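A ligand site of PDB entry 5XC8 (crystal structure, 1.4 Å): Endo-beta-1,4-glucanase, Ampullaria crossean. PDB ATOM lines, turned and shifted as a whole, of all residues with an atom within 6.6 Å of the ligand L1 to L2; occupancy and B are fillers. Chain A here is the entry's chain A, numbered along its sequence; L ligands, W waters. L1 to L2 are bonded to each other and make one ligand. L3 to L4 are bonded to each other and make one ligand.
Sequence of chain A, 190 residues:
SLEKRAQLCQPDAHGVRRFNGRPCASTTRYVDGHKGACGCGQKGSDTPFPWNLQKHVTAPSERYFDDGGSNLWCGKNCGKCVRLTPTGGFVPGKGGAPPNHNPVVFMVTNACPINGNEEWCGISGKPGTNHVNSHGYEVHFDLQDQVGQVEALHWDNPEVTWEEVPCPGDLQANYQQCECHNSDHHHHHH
OD2 of Asp 32 lies within hydrogen-bond range of O2 of LIG L1.
An oxygen (O2) of LIG L1 sits at hydrogen-bond distance from the side-chain amide nitrogen (ND2) of Asn 110.
O of Leu 72 is in hydrogen-bond range of O1 of LG2 L2, at 2.7 Å.
An oxygen (O5) of LG4 L4 sits at hydrogen-bond distance from the side-chain amide oxygen (OD1) of Asn 117.
OD2 of Asp 142 lies within hydrogen-bond range of O3 of LG4 L4 (2.6 Å).
The backbone NH of Gly 36 is in hydrogen-bond range of an oxygen (O5) of LG2 L2.
O5 of LG2 L2 sits at hydrogen-bond distance from OD1 of Asp 46 (2.7 Å).
The indole nitrogen (NE1) of Trp 73 lies within hydrogen-bond range of the side-chain sulfur (SG) of Cys 74 (3.6 Å).
The backbone carbonyl oxygen (O) of Pro 113 sits at hydrogen-bond distance from the side-chain amide nitrogen (ND2) of Asn 117 (3.1 Å).
N of Cys 74 sits at hydrogen-bond distance from O of Ala 37 (2.9 Å).
The side-chain carboxylate of Asp 46 sits at hydrogen-bond distance from the backbone NH of Lys 35.
The side-chain amide nitrogen (ND2) of Asn 110 sits at hydrogen-bond distance from the side-chain hydroxyl (OH) of Tyr 30 (3.0 Å).
The backbone NH of His 34 is in hydrogen-bond range of the side-chain carboxylate of Asp 32 (3.0 Å).
NZ of Lys 35 is in hydrogen-bond range of O of Ser 45, at 2.8 Å.
The side-chain amide oxygen of Asn 110 is in hydrogen-bond range of the backbone NH of Ala 37 (2.9 Å).
O of Ala 111 sits close to O5 of LIG L1 (3.5 Å).
Residues that only touch the ligand L1 to L2: His 34, Lys 35, Ala 37, Trp 73 and Pro 113.
Hydrophobic or aromatic side chains within 4 Å of the ligand L1 to L2: His 34, Ala 37, Leu 72, Trp 73 and Pro 113.
Of the 22 residues printed, 11 come within 4 Å of the ligand L1 to L2.
The nearest printed residue that does not touch the ligand L1 to L2 is Tyr 30 (4.6 Å).
Water W4 bridges the side-chain amide nitrogen of Asn 117 (3.1 Å) and an oxygen (O1) of LIG L1 (3.3 Å).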
ATOM      1  N   TYR A  30     -23.458  26.611  25.593  1.00  0.00           N
ATOM      2  CA  TYR A  30     -22.374  26.336  26.535  1.00  0.00           C
ATOM      3  C   TYR A  30     -21.772  27.617  27.055  1.00  0.00           C
ATOM      4  O   TYR A  30     -21.811  28.664  26.409  1.00  0.00           O
ATOM      5  CB  TYR A  30     -21.261  25.486  25.888  1.00  0.00           C
ATOM      6  CG  TYR A  30     -20.291  26.220  24.964  1.00  0.00           C
ATOM      7  CD1 TYR A  30     -20.591  26.501  23.621  1.00  0.00           C
ATOM      8  CD2 TYR A  30     -19.024  26.509  25.406  1.00  0.00           C
ATOM      9  CE1 TYR A  30     -19.662  27.110  22.770  1.00  0.00           C
ATOM     10  CE2 TYR A  30     -18.070  27.116  24.573  1.00  0.00           C
ATOM     11  CZ  TYR A  30     -18.384  27.412  23.256  1.00  0.00           C
ATOM     12  OH  TYR A  30     -17.411  27.964  22.442  1.00  0.00           O
ATOM     13  N   ASP A  32     -17.964  28.387  29.070  1.00  0.00           N
ATOM     14  CA  ASP A  32     -16.774  27.869  29.744  1.00  0.00           C
ATOM     15  C   ASP A  32     -15.627  28.859  29.893  1.00  0.00           C
ATOM     16  O   ASP A  32     -14.680  28.559  30.629  1.00  0.00           O
ATOM     17  CB  ASP A  32     -16.257  26.528  29.167  1.00  0.00           C
ATOM     18  CG  ASP A  32     -15.717  26.640  27.749  1.00  0.00           C
ATOM     19  OD1 ASP A  32     -15.361  27.746  27.282  1.00  0.00           O
ATOM     20  OD2 ASP A  32     -15.608  25.559  27.129  1.00  0.00           O
ATOM     21  N   GLY A  33     -15.671  30.010  29.184  1.00  0.00           N
ATOM     22  CA  GLY A  33     -14.662  31.046  29.348  1.00  0.00           C
ATOM     23  C   GLY A  33     -13.311  30.786  28.688  1.00  0.00           C
ATOM     24  O   GLY A  33     -12.426  31.652  28.755  1.00  0.00           O
ATOM     25  N   HIS A  34     -13.151  29.662  28.002  1.00  0.00           N
ATOM     26  CA  HIS A  34     -11.868  29.372  27.387  1.00  0.00           C
ATOM     27  C   HIS A  34     -11.681  30.193  26.110  1.00  0.00           C
ATOM     28  O   HIS A  34     -12.628  30.557  25.417  1.00  0.00           O
ATOM     29  CB  HIS A  34     -11.838  27.912  26.972  1.00  0.00           C
ATOM     30  CG  HIS A  34     -11.730  26.987  28.142  1.00  0.00           C
ATOM     31  ND1 HIS A  34     -10.711  27.093  29.065  1.00  0.00           N
ATOM     32  CD2 HIS A  34     -12.514  25.961  28.535  1.00  0.00           C
ATOM     33  CE1 HIS A  34     -10.868  26.150  29.991  1.00  0.00           C
ATOM     34  NE2 HIS A  34     -11.958  25.464  29.691  1.00  0.00           N
ATOM     35  N   LYS A  35     -10.406  30.382  25.739  1.00  0.00           N
ATOM     36  CA  LYS A  35     -10.092  30.985  24.467  1.00  0.00           C
ATOM     37  C   LYS A  35     -10.667  30.170  23.319  1.00  0.00           C
ATOM     38  O   LYS A  35     -11.277  30.720  22.399  1.00  0.00           O
ATOM     39  CB  LYS A  35      -8.567  31.142  24.322  1.00  0.00           C
ATOM     40  CG  LYS A  35      -8.135  31.575  22.916  1.00  0.00           C
ATOM     41  CD  LYS A  35      -6.645  32.012  22.910  1.00  0.00           C
ATOM     42  CE  LYS A  35      -5.739  30.798  23.054  1.00  0.00           C
ATOM     43  NZ  LYS A  35      -4.328  31.333  23.023  1.00  0.00           N
ATOM     44  N   GLY A  36     -10.464  28.857  23.358  1.00  0.00           N
ATOM     45  CA  GLY A  36     -11.081  27.962  22.401  1.00  0.00           C
ATOM     46  C   GLY A  36     -10.123  27.538  21.292  1.00  0.00           C
ATOM     47  O   GLY A  36      -9.001  28.032  21.144  1.00  0.00           O
ATOM     48  N   ALA A  37     -10.614  26.595  20.469  1.00  0.00           N
ATOM     49  CA  ALA A  37      -9.772  25.779  19.603  1.00  0.00           C
ATOM     50  C   ALA A  37      -9.379  26.462  18.316  1.00  0.00           C
ATOM     51  O   ALA A  37      -8.578  25.885  17.537  1.00  0.00           O
ATOM     52  CB  ALA A  37     -10.505  24.455  19.308  1.00  0.00           C
ATOM     53  N   CYS A  38      -9.874  27.676  18.046  1.00  0.00           N
ATOM     54  CA  CYS A  38      -9.416  28.441  16.886  1.00  0.00           C
ATOM     55  C   CYS A  38      -8.499  29.581  17.281  1.00  0.00           C
ATOM     56  O   CYS A  38      -8.092  30.382  16.418  1.00  0.00           O
ATOM     57  CB  CYS A  38     -10.584  28.953  16.028  1.00  0.00           C
ATOM     58  SG  CYS A  38     -11.646  27.617  15.386  1.00  0.00           S
ATOM     59  N   GLY A  39      -8.083  29.645  18.547  1.00  0.00           N
ATOM     60  CA  GLY A  39      -7.083  30.625  18.910  1.00  0.00           C
ATOM     61  C   GLY A  39      -7.593  32.058  18.905  1.00  0.00           C
ATOM     62  O   GLY A  39      -6.802  32.984  18.715  1.00  0.00           O
ATOM     63  N   SER A  45      -2.084  32.451  25.984  1.00  0.00           N
ATOM     64  CA  SER A  45      -2.932  32.601  27.163  1.00  0.00           C
ATOM     65  C   SER A  45      -4.271  31.929  26.859  1.00  0.00           C
ATOM     66  O   SER A  45      -4.659  31.828  25.709  1.00  0.00           O
ATOM     67  CB  SER A  45      -3.300  34.065  27.367  1.00  0.00           C
ATOM     68  OG  SER A  45      -4.431  34.366  26.553  1.00  0.00           O
ATOM     69  N   ASP A  46      -4.981  31.506  27.895  1.00  0.00           N
ATOM     70  CA  ASP A  46      -6.331  30.972  27.713  1.00  0.00           C
ATOM     71  C   ASP A  46      -7.384  32.069  27.859  1.00  0.00           C
ATOM     72  O   ASP A  46      -8.428  31.840  28.455  1.00  0.00           O
ATOM     73  CB  ASP A  46      -6.598  29.844  28.700  1.00  0.00           C
ATOM     74  CG  ASP A  46      -7.841  29.048  28.350  1.00  0.00           C
ATOM     75  OD1 ASP A  46      -8.190  28.996  27.175  1.00  0.00           O
ATOM     76  OD2 ASP A  46      -8.495  28.519  29.262  1.00  0.00           O
ATOM     77  N   THR A  47      -7.130  33.246  27.317  1.00  0.00           N
ATOM     78  CA  THR A  47      -8.046  34.380  27.455  1.00  0.00           C
ATOM     79  C   THR A  47      -8.665  34.696  26.104  1.00  0.00           C
ATOM     80  O   THR A  47      -7.955  35.118  25.191  1.00  0.00           O
ATOM     81  CB  THR A  47      -7.238  35.588  27.948  1.00  0.00           C
ATOM     82  OG1 THR A  47      -6.586  35.244  29.172  1.00  0.00           O
ATOM     83  CG2 THR A  47      -8.103  36.820  28.177  1.00  0.00           C
ATOM     84  N   ALA A  59     -19.193  26.236  18.602  1.00  0.00           N
ATOM     85  CA  ALA A  59     -18.280  25.094  18.670  1.00  0.00           C
ATOM     86  C   ALA A  59     -19.019  23.923  18.024  1.00  0.00           C
ATOM     87  O   ALA A  59     -19.850  23.286  18.683  1.00  0.00           O
ATOM     88  CB  ALA A  59     -17.973  24.779  20.135  1.00  0.00           C
ATOM     89  N   LEU A  72      -7.861  19.256  17.341  1.00  0.00           N
ATOM     90  CA  LEU A  72      -8.660  20.150  18.201  1.00  0.00           C
ATOM     91  C   LEU A  72      -7.944  21.471  18.411  1.00  0.00           C
ATOM     92  O   LEU A  72      -8.201  22.177  19.392  1.00  0.00           O
ATOM     93  CB  LEU A  72      -8.984  19.473  19.525  1.00  0.00           C
ATOM     94  CG  LEU A  72      -9.885  18.223  19.396  1.00  0.00           C
ATOM     95  CD1 LEU A  72     -10.008  17.536  20.750  1.00  0.00           C
ATOM     96  CD2 LEU A  72     -11.254  18.667  18.925  1.00  0.00           C
ATOM     97  N   TRP A  73      -7.082  21.839  17.473  1.00  0.00           N
ATOM     98  CA  TRP A  73      -6.419  23.153  17.468  1.00  0.00           C
ATOM     99  C   TRP A  73      -6.262  23.546  16.004  1.00  0.00           C
ATOM    100  O   TRP A  73      -5.702  22.778  15.215  1.00  0.00           O
ATOM    101  CB  TRP A  73      -5.063  23.086  18.165  1.00  0.00           C
ATOM    102  CG  TRP A  73      -4.257  24.361  18.086  1.00  0.00           C
ATOM    103  CD1 TRP A  73      -3.114  24.563  17.361  1.00  0.00           C
ATOM    104  CD2 TRP A  73      -4.541  25.627  18.740  1.00  0.00           C
ATOM    105  NE1 TRP A  73      -2.665  25.848  17.525  1.00  0.00           N
ATOM    106  CE2 TRP A  73      -3.523  26.526  18.350  1.00  0.00           C
ATOM    107  CE3 TRP A  73      -5.549  26.084  19.599  1.00  0.00           C
ATOM    108  CZ2 TRP A  73      -3.453  27.822  18.802  1.00  0.00           C
ATOM    109  CZ3 TRP A  73      -5.488  27.419  20.042  1.00  0.00           C
ATOM    110  CH2 TRP A  73      -4.416  28.257  19.647  1.00  0.00           C
ATOM    111  N   CYS A  74      -6.823  24.696  15.632  1.00  0.00           N
ATOM    112  CA  CYS A  74      -6.809  25.169  14.245  1.00  0.00           C
ATOM    113  C   CYS A  74      -7.402  24.126  13.317  1.00  0.00           C
ATOM    114  O   CYS A  74      -6.793  23.696  12.315  1.00  0.00           O
ATOM    115  CB  CYS A  74      -5.420  25.590  13.734  1.00  0.00           C
ATOM    116  SG  CYS A  74      -4.680  26.924  14.763  1.00  0.00           S
ATOM    117  N   ASN A 110     -14.594  27.463  17.901  1.00  0.00           N
ATOM    118  CA  ASN A 110     -14.223  26.511  18.926  1.00  0.00           C
ATOM    119  C   ASN A 110     -14.696  25.147  18.453  1.00  0.00           C
ATOM    120  O   ASN A 110     -15.276  25.034  17.368  1.00  0.00           O
ATOM    121  CB  ASN A 110     -14.817  26.965  20.275  1.00  0.00           C
ATOM    122  CG  ASN A 110     -14.215  26.283  21.465  1.00  0.00           C
ATOM    123  OD1 ASN A 110     -13.187  25.603  21.389  1.00  0.00           O
ATOM    124  ND2 ASN A 110     -14.861  26.482  22.603  1.00  0.00           N
ATOM    125  N   ALA A 111     -14.442  24.092  19.251  1.00  0.00           N
ATOM    126  CA  ALA A 111     -14.806  22.730  18.901  1.00  0.00           C
ATOM    127  C   ALA A 111     -15.547  22.083  20.051  1.00  0.00           C
ATOM    128  O   ALA A 111     -15.255  22.331  21.226  1.00  0.00           O
ATOM    129  CB  ALA A 111     -13.545  21.876  18.623  1.00  0.00           C
ATOM    130  N   CYS A 112     -16.489  21.196  19.712  1.00  0.00           N
ATOM    131  CA  CYS A 112     -17.163  20.334  20.673  1.00  0.00           C
ATOM    132  C   CYS A 112     -16.621  18.926  20.501  1.00  0.00           C
ATOM    133  O   CYS A 112     -16.991  18.223  19.541  1.00  0.00           O
ATOM    134  CB  CYS A 112     -18.661  20.355  20.352  1.00  0.00           C
ATOM    135  SG  CYS A 112     -19.615  19.347  21.590  1.00  0.00           S
ATOM    136  N   PRO A 113     -15.698  18.498  21.378  1.00  0.00           N
ATOM    137  CA  PRO A 113     -15.037  17.194  21.150  1.00  0.00           C
ATOM    138  C   PRO A 113     -15.975  16.035  21.452  1.00  0.00           C
ATOM    139  O   PRO A 113     -16.904  16.136  22.246  1.00  0.00           O
ATOM    140  CB  PRO A 113     -13.885  17.224  22.161  1.00  0.00           C
ATOM    141  CG  PRO A 113     -14.348  18.191  23.223  1.00  0.00           C
ATOM    142  CD  PRO A 113     -15.188  19.214  22.560  1.00  0.00           C
ATOM    143  N   ASN A 117     -18.734  14.606  25.335  1.00  0.00           N
ATOM    144  CA  ASN A 117     -19.941  15.139  24.724  1.00  0.00           C
ATOM    145  C   ASN A 117     -20.530  14.108  23.791  1.00  0.00           C
ATOM    146  O   ASN A 117     -20.893  14.394  22.653  1.00  0.00           O
ATOM    147  CB  ASN A 117     -19.632  16.426  23.960  1.00  0.00           C
ATOM    148  CG  ASN A 117     -19.061  17.489  24.857  1.00  0.00           C
ATOM    149  OD1 ASN A 117     -19.787  18.121  25.619  1.00  0.00           O
ATOM    150  ND2 ASN A 117     -17.779  17.701  24.761  1.00  0.00           N
ATOM    151  N   ASP A 142     -22.768  23.711  19.150  1.00  0.00           N
ATOM    152  CA  ASP A 142     -22.859  24.175  20.543  1.00  0.00           C
ATOM    153  C   ASP A 142     -22.675  25.683  20.468  1.00  0.00           C
ATOM    154  O   ASP A 142     -21.696  26.164  19.888  1.00  0.00           O
ATOM    155  CB  ASP A 142     -21.765  23.474  21.339  1.00  0.00           C
ATOM    156  CG  ASP A 142     -22.025  23.419  22.826  1.00  0.00           C
ATOM    157  OD1 ASP A 142     -23.115  23.739  23.277  1.00  0.00           O
ATOM    158  OD2 ASP A 142     -21.077  23.037  23.555  1.00  0.00           O
HETATM  159  C1  LIG L   1     -13.107  24.220  24.987  1.00  0.00           C
HETATM  160  C2  LIG L   1     -11.837  24.516  24.208  1.00  0.00           C
HETATM  161  C3  LIG L   1     -11.144  23.212  23.823  1.00  0.00           C
HETATM  162  C4  LIG L   1     -12.110  22.282  23.101  1.00  0.00           C
HETATM  163  C5  LIG L   1     -11.505  20.945  22.654  1.00  0.00           C
HETATM  164  C6  LIG L   1     -13.950  23.183  24.224  1.00  0.00           C
HETATM  165  O1  LIG L   1     -15.096  22.770  25.015  1.00  0.00           O
HETATM  166  O2  LIG L   1     -13.843  25.435  25.123  1.00  0.00           O
HETATM  167  O3  LIG L   1     -11.001  25.292  25.116  1.00  0.00           O
HETATM  168  O4  LIG L   1     -10.135  23.496  22.841  1.00  0.00           O
HETATM  169  O5  LIG L   1     -13.173  22.000  24.000  1.00  0.00           O
HETATM  170  O6  LIG L   1     -11.007  20.238  23.791  1.00  0.00           O
HETATM  171  C1  LG2 L   2      -7.816  23.372  22.307  1.00  0.00           C
HETATM  172  C2  LG2 L   2      -6.440  23.662  22.872  1.00  0.00           C
HETATM  173  C3  LG2 L   2      -6.351  25.144  23.224  1.00  0.00           C
HETATM  174  C4  LG2 L   2      -7.495  25.552  24.145  1.00  0.00           C
HETATM  175  C5  LG2 L   2      -7.543  27.068  24.319  1.00  0.00           C
HETATM  176  C6  LG2 L   2      -8.838  23.778  23.333  1.00  0.00           C
HETATM  177  O1  LG2 L   2      -7.938  21.959  22.086  1.00  0.00           O
HETATM  178  O2  LG2 L   2      -5.433  23.341  21.908  1.00  0.00           O
HETATM  179  O3  LG2 L   2      -5.108  25.410  23.916  1.00  0.00           O
HETATM  180  O4  LG2 L   2      -8.728  25.206  23.482  1.00  0.00           O
HETATM  181  O5  LG2 L   2      -8.731  27.375  25.082  1.00  0.00           O
HETATM  182  C1  LG3 L   3     -29.022  19.108  27.449  1.00  0.00           C
HETATM  183  C2  LG3 L   3     -27.550  19.318  27.786  1.00  0.00           C
HETATM  184  C3  LG3 L   3     -27.060  20.683  27.327  1.00  0.00           C
HETATM  185  C4  LG3 L   3     -28.039  21.740  27.848  1.00  0.00           C
HETATM  186  C5  LG3 L   3     -27.822  23.144  27.347  1.00  0.00           C
HETATM  187  C6  LG3 L   3     -29.829  20.220  28.039  1.00  0.00           C
HETATM  188  O1  LG3 L   3     -31.206  20.134  27.651  1.00  0.00           O
HETATM  189  O2  LG3 L   3     -29.602  17.919  28.038  1.00  0.00           O
HETATM  190  O3  LG3 L   3     -26.791  18.280  27.159  1.00  0.00           O
HETATM  191  O4  LG3 L   3     -25.784  20.914  27.938  1.00  0.00           O
HETATM  192  O5  LG3 L   3     -29.358  21.406  27.450  1.00  0.00           O
HETATM  193  O6  LG3 L   3     -27.744  23.171  25.936  1.00  0.00           O
HETATM  194  C1  LG4 L   4     -23.691  21.973  27.938  1.00  0.00           C
HETATM  195  C2  LG4 L   4     -22.435  22.219  27.141  1.00  0.00           C
HETATM  196  C3  LG4 L   4     -22.043  20.980  26.342  1.00  0.00           C
HETATM  197  C4  LG4 L   4     -23.220  20.651  25.442  1.00  0.00           C
HETATM  198  C5  LG4 L   4     -22.994  19.470  24.502  1.00  0.00           C
HETATM  199  C6  LG4 L   4     -24.768  21.387  27.059  1.00  0.00           C
HETATM  200  O1  LG4 L   4     -24.162  23.216  28.511  1.00  0.00           O
HETATM  201  O2  LG4 L   4     -21.402  22.591  28.107  1.00  0.00           O
HETATM  202  O3  LG4 L   4     -20.918  21.337  25.530  1.00  0.00           O
HETATM  203  O4  LG4 L   4     -24.295  20.285  26.298  1.00  0.00           O
HETATM  204  O5  LG4 L   4     -22.551  18.339  25.249  1.00  0.00           O
HETATM  205  O   HOH W   1      -4.863  24.151  26.371  1.00  0.00           O
HETATM  206  O   HOH W   2      -5.005  20.646  21.167  1.00  0.00           O
HETATM  207  O   HOH W   3      -9.680  23.962  27.318  1.00  0.00           O
HETATM  208  O   HOH W   4     -16.003  19.774  26.203  1.00  0.00           O
